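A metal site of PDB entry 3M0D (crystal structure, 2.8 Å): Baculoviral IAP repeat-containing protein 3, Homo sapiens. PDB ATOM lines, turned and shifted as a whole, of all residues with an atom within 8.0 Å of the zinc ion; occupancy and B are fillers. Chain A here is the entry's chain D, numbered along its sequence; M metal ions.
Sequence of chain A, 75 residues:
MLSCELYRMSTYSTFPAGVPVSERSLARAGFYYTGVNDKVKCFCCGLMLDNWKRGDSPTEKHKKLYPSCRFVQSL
Of the 22 residues printed, 4 come within 4 Å of the zinc ion.
A ring nitrogen (NE2) of His 62 is bound to the zinc ion, 2.1 Å away.
SG of Cys 42 is bound to the zinc ion (2.3 Å).
The zinc ion is bound by SG of Cys 69 (2.4 Å).
The side-chain sulfur (SG) of Cys 45 binds the zinc ion (2.4 Å).
The zinc ion has four donor atoms within binding distance.
SG of Cys 69 lies close to N of Phe 71 (3.4 Å).
SG of Cys 45 lies close to N of Leu 47, 3.4 Å away.
The side-chain sulfur (SG) of Cys 69 sits close to the side-chain sulfur (SG) of Cys 44 (3.6 Å).
The backbone NH (N) of Cys 42 lies within hydrogen-bond range of the backbone carbonyl oxygen (O) of Leu 47 (3.0 Å).
The backbone carbonyl oxygen (O) of Ala 29 sits at hydrogen-bond distance from a ring nitrogen (ND1) of His 62 (2.9 Å).
SG of Cys 69 lies close to N of Val 72, at 3.5 Å.
N of Cys 44 lies close to SG of Cys 42 (3.2 Å).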
ATOM      1  N   ALA A  29      25.545 -33.523 -17.844  1.00  0.00           N
ATOM      2  CA  ALA A  29      25.007 -32.879 -19.036  1.00  0.00           C
ATOM      3  C   ALA A  29      24.137 -31.669 -18.730  1.00  0.00           C
ATOM      4  O   ALA A  29      23.567 -31.073 -19.650  1.00  0.00           O
ATOM      5  CB  ALA A  29      24.215 -33.882 -19.866  1.00  0.00           C
ATOM      6  N   GLY A  30      24.024 -31.327 -17.451  1.00  0.00           N
ATOM      7  CA  GLY A  30      23.324 -30.118 -17.023  1.00  0.00           C
ATOM      8  C   GLY A  30      21.844 -30.258 -16.679  1.00  0.00           C
ATOM      9  O   GLY A  30      21.155 -29.239 -16.482  1.00  0.00           O
ATOM     10  N   PHE A  31      21.350 -31.482 -16.600  1.00  0.00           N
ATOM     11  CA  PHE A  31      19.937 -31.716 -16.327  1.00  0.00           C
ATOM     12  C   PHE A  31      19.678 -32.142 -14.890  1.00  0.00           C
ATOM     13  O   PHE A  31      20.453 -32.929 -14.309  1.00  0.00           O
ATOM     14  CB  PHE A  31      19.387 -32.802 -17.258  1.00  0.00           C
ATOM     15  CG  PHE A  31      19.540 -32.505 -18.715  1.00  0.00           C
ATOM     16  CD1 PHE A  31      18.744 -31.537 -19.329  1.00  0.00           C
ATOM     17  CD2 PHE A  31      20.465 -33.210 -19.493  1.00  0.00           C
ATOM     18  CE1 PHE A  31      18.878 -31.254 -20.697  1.00  0.00           C
ATOM     19  CE2 PHE A  31      20.599 -32.937 -20.851  1.00  0.00           C
ATOM     20  CZ  PHE A  31      19.804 -31.961 -21.445  1.00  0.00           C
ATOM     21  N   LYS A  41      15.561 -31.841 -16.854  1.00  0.00           N
ATOM     22  CA  LYS A  41      15.434 -30.466 -17.280  1.00  0.00           C
ATOM     23  C   LYS A  41      16.771 -29.730 -17.098  1.00  0.00           C
ATOM     24  O   LYS A  41      17.433 -29.870 -16.041  1.00  0.00           O
ATOM     25  CB  LYS A  41      14.325 -29.782 -16.482  1.00  0.00           C
ATOM     26  CG  LYS A  41      13.732 -28.548 -17.151  1.00  0.00           C
ATOM     27  CD  LYS A  41      12.493 -28.087 -16.394  1.00  0.00           C
ATOM     28  CE  LYS A  41      12.134 -26.632 -16.670  1.00  0.00           C
ATOM     29  NZ  LYS A  41      11.643 -26.404 -18.055  1.00  0.00           N
ATOM     30  N   CYS A  42      17.182 -28.968 -18.124  1.00  0.00           N
ATOM     31  CA  CYS A  42      18.324 -28.079 -17.973  1.00  0.00           C
ATOM     32  C   CYS A  42      17.941 -26.881 -17.119  1.00  0.00           C
ATOM     33  O   CYS A  42      17.014 -26.132 -17.454  1.00  0.00           O
ATOM     34  CB  CYS A  42      18.841 -27.596 -19.323  1.00  0.00           C
ATOM     35  SG  CYS A  42      20.240 -26.405 -19.099  1.00  0.00           S
ATOM     36  N   PHE A  43      18.647 -26.706 -15.996  1.00  0.00           N
ATOM     37  CA  PHE A  43      18.373 -25.585 -15.086  1.00  0.00           C
ATOM     38  C   PHE A  43      18.398 -24.276 -15.873  1.00  0.00           C
ATOM     39  O   PHE A  43      17.659 -23.345 -15.585  1.00  0.00           O
ATOM     40  CB  PHE A  43      19.378 -25.558 -13.911  1.00  0.00           C
ATOM     41  CG  PHE A  43      20.841 -25.401 -14.320  1.00  0.00           C
ATOM     42  CD1 PHE A  43      21.471 -24.175 -14.222  1.00  0.00           C
ATOM     43  CD2 PHE A  43      21.568 -26.478 -14.802  1.00  0.00           C
ATOM     44  CE1 PHE A  43      22.804 -24.020 -14.608  1.00  0.00           C
ATOM     45  CE2 PHE A  43      22.898 -26.336 -15.192  1.00  0.00           C
ATOM     46  CZ  PHE A  43      23.511 -25.106 -15.090  1.00  0.00           C
ATOM     47  N   CYS A  44      19.225 -24.259 -16.901  1.00  0.00           N
ATOM     48  CA  CYS A  44      19.665 -23.049 -17.567  1.00  0.00           C
ATOM     49  C   CYS A  44      18.778 -22.662 -18.753  1.00  0.00           C
ATOM     50  O   CYS A  44      18.085 -21.645 -18.696  1.00  0.00           O
ATOM     51  CB  CYS A  44      21.123 -23.241 -17.994  1.00  0.00           C
ATOM     52  SG  CYS A  44      21.847 -21.865 -18.832  1.00  0.00           S
ATOM     53  N   CYS A  45      18.786 -23.448 -19.833  1.00  0.00           N
ATOM     54  CA  CYS A  45      17.945 -23.146 -20.995  1.00  0.00           C
ATOM     55  C   CYS A  45      16.506 -23.668 -20.819  1.00  0.00           C
ATOM     56  O   CYS A  45      15.565 -23.155 -21.436  1.00  0.00           O
ATOM     57  CB  CYS A  45      18.572 -23.687 -22.291  1.00  0.00           C
ATOM     58  SG  CYS A  45      18.377 -25.469 -22.573  1.00  0.00           S
ATOM     59  N   GLY A  46      16.345 -24.696 -19.990  1.00  0.00           N
ATOM     60  CA  GLY A  46      15.035 -25.246 -19.712  1.00  0.00           C
ATOM     61  C   GLY A  46      14.571 -26.319 -20.678  1.00  0.00           C
ATOM     62  O   GLY A  46      13.395 -26.693 -20.695  1.00  0.00           O
ATOM     63  N   LEU A  47      15.493 -26.808 -21.502  1.00  0.00           N
ATOM     64  CA  LEU A  47      15.200 -27.938 -22.365  1.00  0.00           C
ATOM     65  C   LEU A  47      14.792 -29.118 -21.474  1.00  0.00           C
ATOM     66  O   LEU A  47      15.505 -29.450 -20.531  1.00  0.00           O
ATOM     67  CB  LEU A  47      16.442 -28.289 -23.179  1.00  0.00           C
ATOM     68  CG  LEU A  47      16.349 -29.472 -24.143  1.00  0.00           C
ATOM     69  CD1 LEU A  47      15.489 -29.126 -25.352  1.00  0.00           C
ATOM     70  CD2 LEU A  47      17.742 -29.890 -24.570  1.00  0.00           C
ATOM     71  N   MET A  48      13.648 -29.724 -21.788  1.00  0.00           N
ATOM     72  CA  MET A  48      13.195 -30.947 -21.116  1.00  0.00           C
ATOM     73  C   MET A  48      13.296 -32.131 -22.061  1.00  0.00           C
ATOM     74  O   MET A  48      12.917 -31.998 -23.230  1.00  0.00           O
ATOM     75  CB  MET A  48      11.750 -30.811 -20.645  1.00  0.00           C
ATOM     76  CG  MET A  48      11.529 -29.850 -19.497  1.00  0.00           C
ATOM     77  SD  MET A  48       9.795 -29.336 -19.414  1.00  0.00           S
ATOM     78  CE  MET A  48       9.636 -28.369 -20.915  1.00  0.00           C
ATOM     79  N   HIS A  62      21.927 -32.350 -25.729  1.00  0.00           N
ATOM     80  CA  HIS A  62      21.755 -31.001 -25.173  1.00  0.00           C
ATOM     81  C   HIS A  62      22.353 -29.953 -26.095  1.00  0.00           C
ATOM     82  O   HIS A  62      21.772 -28.870 -26.254  1.00  0.00           O
ATOM     83  CB  HIS A  62      22.391 -30.899 -23.785  1.00  0.00           C
ATOM     84  CG  HIS A  62      21.942 -29.695 -23.003  1.00  0.00           C
ATOM     85  ND1 HIS A  62      22.312 -29.480 -21.692  1.00  0.00           N
ATOM     86  CD2 HIS A  62      21.145 -28.654 -23.346  1.00  0.00           C
ATOM     87  CE1 HIS A  62      21.771 -28.349 -21.259  1.00  0.00           C
ATOM     88  NE2 HIS A  62      21.060 -27.834 -22.242  1.00  0.00           N
ATOM     89  N   LYS A  63      23.508 -30.266 -26.681  1.00  0.00           N
ATOM     90  CA  LYS A  63      24.164 -29.381 -27.643  1.00  0.00           C
ATOM     91  C   LYS A  63      23.327 -29.254 -28.924  1.00  0.00           C
ATOM     92  O   LYS A  63      23.202 -28.166 -29.479  1.00  0.00           O
ATOM     93  CB  LYS A  63      25.600 -29.846 -27.941  1.00  0.00           C
ATOM     94  N   LEU A  65      19.846 -29.985 -29.500  1.00  0.00           N
ATOM     95  CA  LEU A  65      18.483 -29.489 -29.386  1.00  0.00           C
ATOM     96  C   LEU A  65      18.358 -28.075 -28.788  1.00  0.00           C
ATOM     97  O   LEU A  65      17.248 -27.547 -28.679  1.00  0.00           O
ATOM     98  CB  LEU A  65      17.622 -30.475 -28.608  1.00  0.00           C
ATOM     99  CG  LEU A  65      17.465 -31.827 -29.299  1.00  0.00           C
ATOM    100  CD1 LEU A  65      17.114 -32.946 -28.317  1.00  0.00           C
ATOM    101  CD2 LEU A  65      16.424 -31.721 -30.412  1.00  0.00           C
ATOM    102  N   TYR A  66      19.497 -27.479 -28.412  1.00  0.00           N
ATOM    103  CA  TYR A  66      19.521 -26.133 -27.808  1.00  0.00           C
ATOM    104  C   TYR A  66      20.938 -25.557 -27.673  1.00  0.00           C
ATOM    105  O   TYR A  66      21.415 -25.320 -26.554  1.00  0.00           O
ATOM    106  CB  TYR A  66      18.866 -26.166 -26.431  1.00  0.00           C
ATOM    107  CG  TYR A  66      18.145 -24.905 -26.073  1.00  0.00           C
ATOM    108  CD1 TYR A  66      16.763 -24.888 -25.921  1.00  0.00           C
ATOM    109  CD2 TYR A  66      18.838 -23.716 -25.875  1.00  0.00           C
ATOM    110  CE1 TYR A  66      16.092 -23.723 -25.583  1.00  0.00           C
ATOM    111  CE2 TYR A  66      18.178 -22.532 -25.536  1.00  0.00           C
ATOM    112  CZ  TYR A  66      16.797 -22.551 -25.392  1.00  0.00           C
ATOM    113  OH  TYR A  66      16.121 -21.400 -25.058  1.00  0.00           O
ATOM    114  N   PRO A  67      21.608 -25.313 -28.816  1.00  0.00           N
ATOM    115  CA  PRO A  67      23.024 -24.922 -28.864  1.00  0.00           C
ATOM    116  C   PRO A  67      23.240 -23.572 -28.205  1.00  0.00           C
ATOM    117  O   PRO A  67      24.371 -23.144 -27.931  1.00  0.00           O
ATOM    118  CB  PRO A  67      23.313 -24.814 -30.365  1.00  0.00           C
ATOM    119  CG  PRO A  67      22.181 -25.533 -31.035  1.00  0.00           C
ATOM    120  CD  PRO A  67      20.997 -25.323 -30.153  1.00  0.00           C
ATOM    121  N   SER A  68      22.117 -22.907 -27.945  1.00  0.00           N
ATOM    122  CA  SER A  68      22.109 -21.566 -27.391  1.00  0.00           C
ATOM    123  C   SER A  68      22.292 -21.549 -25.855  1.00  0.00           C
ATOM    124  O   SER A  68      22.522 -20.501 -25.265  1.00  0.00           O
ATOM    125  CB  SER A  68      20.794 -20.898 -27.770  1.00  0.00           C
ATOM    126  OG  SER A  68      20.753 -19.571 -27.286  1.00  0.00           O
ATOM    127  N   CYS A  69      22.176 -22.710 -25.225  1.00  0.00           N
ATOM    128  CA  CYS A  69      22.239 -22.781 -23.781  1.00  0.00           C
ATOM    129  C   CYS A  69      23.559 -22.292 -23.251  1.00  0.00           C
ATOM    130  O   CYS A  69      24.584 -22.829 -23.596  1.00  0.00           O
ATOM    131  CB  CYS A  69      21.991 -24.197 -23.291  1.00  0.00           C
ATOM    132  SG  CYS A  69      22.003 -24.339 -21.476  1.00  0.00           S
ATOM    133  N   ARG A  70      23.512 -21.299 -22.377  1.00  0.00           N
ATOM    134  CA  ARG A  70      24.722 -20.791 -21.736  1.00  0.00           C
ATOM    135  C   ARG A  70      25.539 -21.912 -21.101  1.00  0.00           C
ATOM    136  O   ARG A  70      26.771 -21.930 -21.210  1.00  0.00           O
ATOM    137  CB  ARG A  70      24.355 -19.734 -20.690  1.00  0.00           C
ATOM    138  CG  ARG A  70      25.532 -18.879 -20.184  1.00  0.00           C
ATOM    139  CD  ARG A  70      26.170 -19.486 -18.947  1.00  0.00           C
ATOM    140  NE  ARG A  70      25.259 -19.509 -17.803  1.00  0.00           N
ATOM    141  CZ  ARG A  70      25.485 -20.184 -16.672  1.00  0.00           C
ATOM    142  NH1 ARG A  70      26.589 -20.906 -16.520  1.00  0.00           N
ATOM    143  NH2 ARG A  70      24.594 -20.140 -15.696  1.00  0.00           N
ATOM    144  N   PHE A  71      24.853 -22.857 -20.448  1.00  0.00           N
ATOM    145  CA  PHE A  71      25.543 -23.975 -19.806  1.00  0.00           C
ATOM    146  C   PHE A  71      26.174 -24.908 -20.839  1.00  0.00           C
ATOM    147  O   PHE A  71      27.341 -25.280 -20.731  1.00  0.00           O
ATOM    148  CB  PHE A  71      24.619 -24.798 -18.905  1.00  0.00           C
ATOM    149  CG  PHE A  71      25.265 -26.082 -18.437  1.00  0.00           C
ATOM    150  CD1 PHE A  71      26.052 -26.101 -17.302  1.00  0.00           C
ATOM    151  CD2 PHE A  71      25.136 -27.257 -19.183  1.00  0.00           C
ATOM    152  CE1 PHE A  71      26.682 -27.265 -16.881  1.00  0.00           C
ATOM    153  CE2 PHE A  71      25.764 -28.429 -18.782  1.00  0.00           C
ATOM    154  CZ  PHE A  71      26.543 -28.429 -17.626  1.00  0.00           C
ATOM    155  N   VAL A  72      25.366 -25.304 -21.811  1.00  0.00           N
ATOM    156  CA  VAL A  72      25.786 -26.264 -22.800  1.00  0.00           C
ATOM    157  C   VAL A  72      26.941 -25.695 -23.634  1.00  0.00           C
ATOM    158  O   VAL A  72      27.636 -26.429 -24.318  1.00  0.00           O
ATOM    159  CB  VAL A  72      24.587 -26.707 -23.665  1.00  0.00           C
ATOM    160  CG1 VAL A  72      24.484 -25.885 -24.955  1.00  0.00           C
ATOM    161  CG2 VAL A  72      24.690 -28.192 -23.952  1.00  0.00           C
ATOM    162  N   GLN A  73      27.162 -24.383 -23.544  1.00  0.00           N
ATOM    163  CA  GLN A  73      28.296 -23.760 -24.225  1.00  0.00           C
ATOM    164  C   GLN A  73      29.622 -23.847 -23.445  1.00  0.00           C
ATOM    165  O   GLN A  73      30.690 -23.868 -24.050  1.00  0.00           O
ATOM    166  CB  GLN A  73      27.989 -22.315 -24.656  1.00  0.00           C
ATOM    167  CG  GLN A  73      27.222 -22.227 -25.988  1.00  0.00           C
ATOM    168  CD  GLN A  73      27.084 -20.804 -26.531  1.00  0.00           C
ATOM    169  OE1 GLN A  73      28.016 -20.016 -26.480  1.00  0.00           O
ATOM    170  NE2 GLN A  73      25.910 -20.500 -27.073  1.00  0.00           N
HETATM  171 ZN    ZN M   1      20.367 -26.041 -21.390  1.00  0.00          ZN
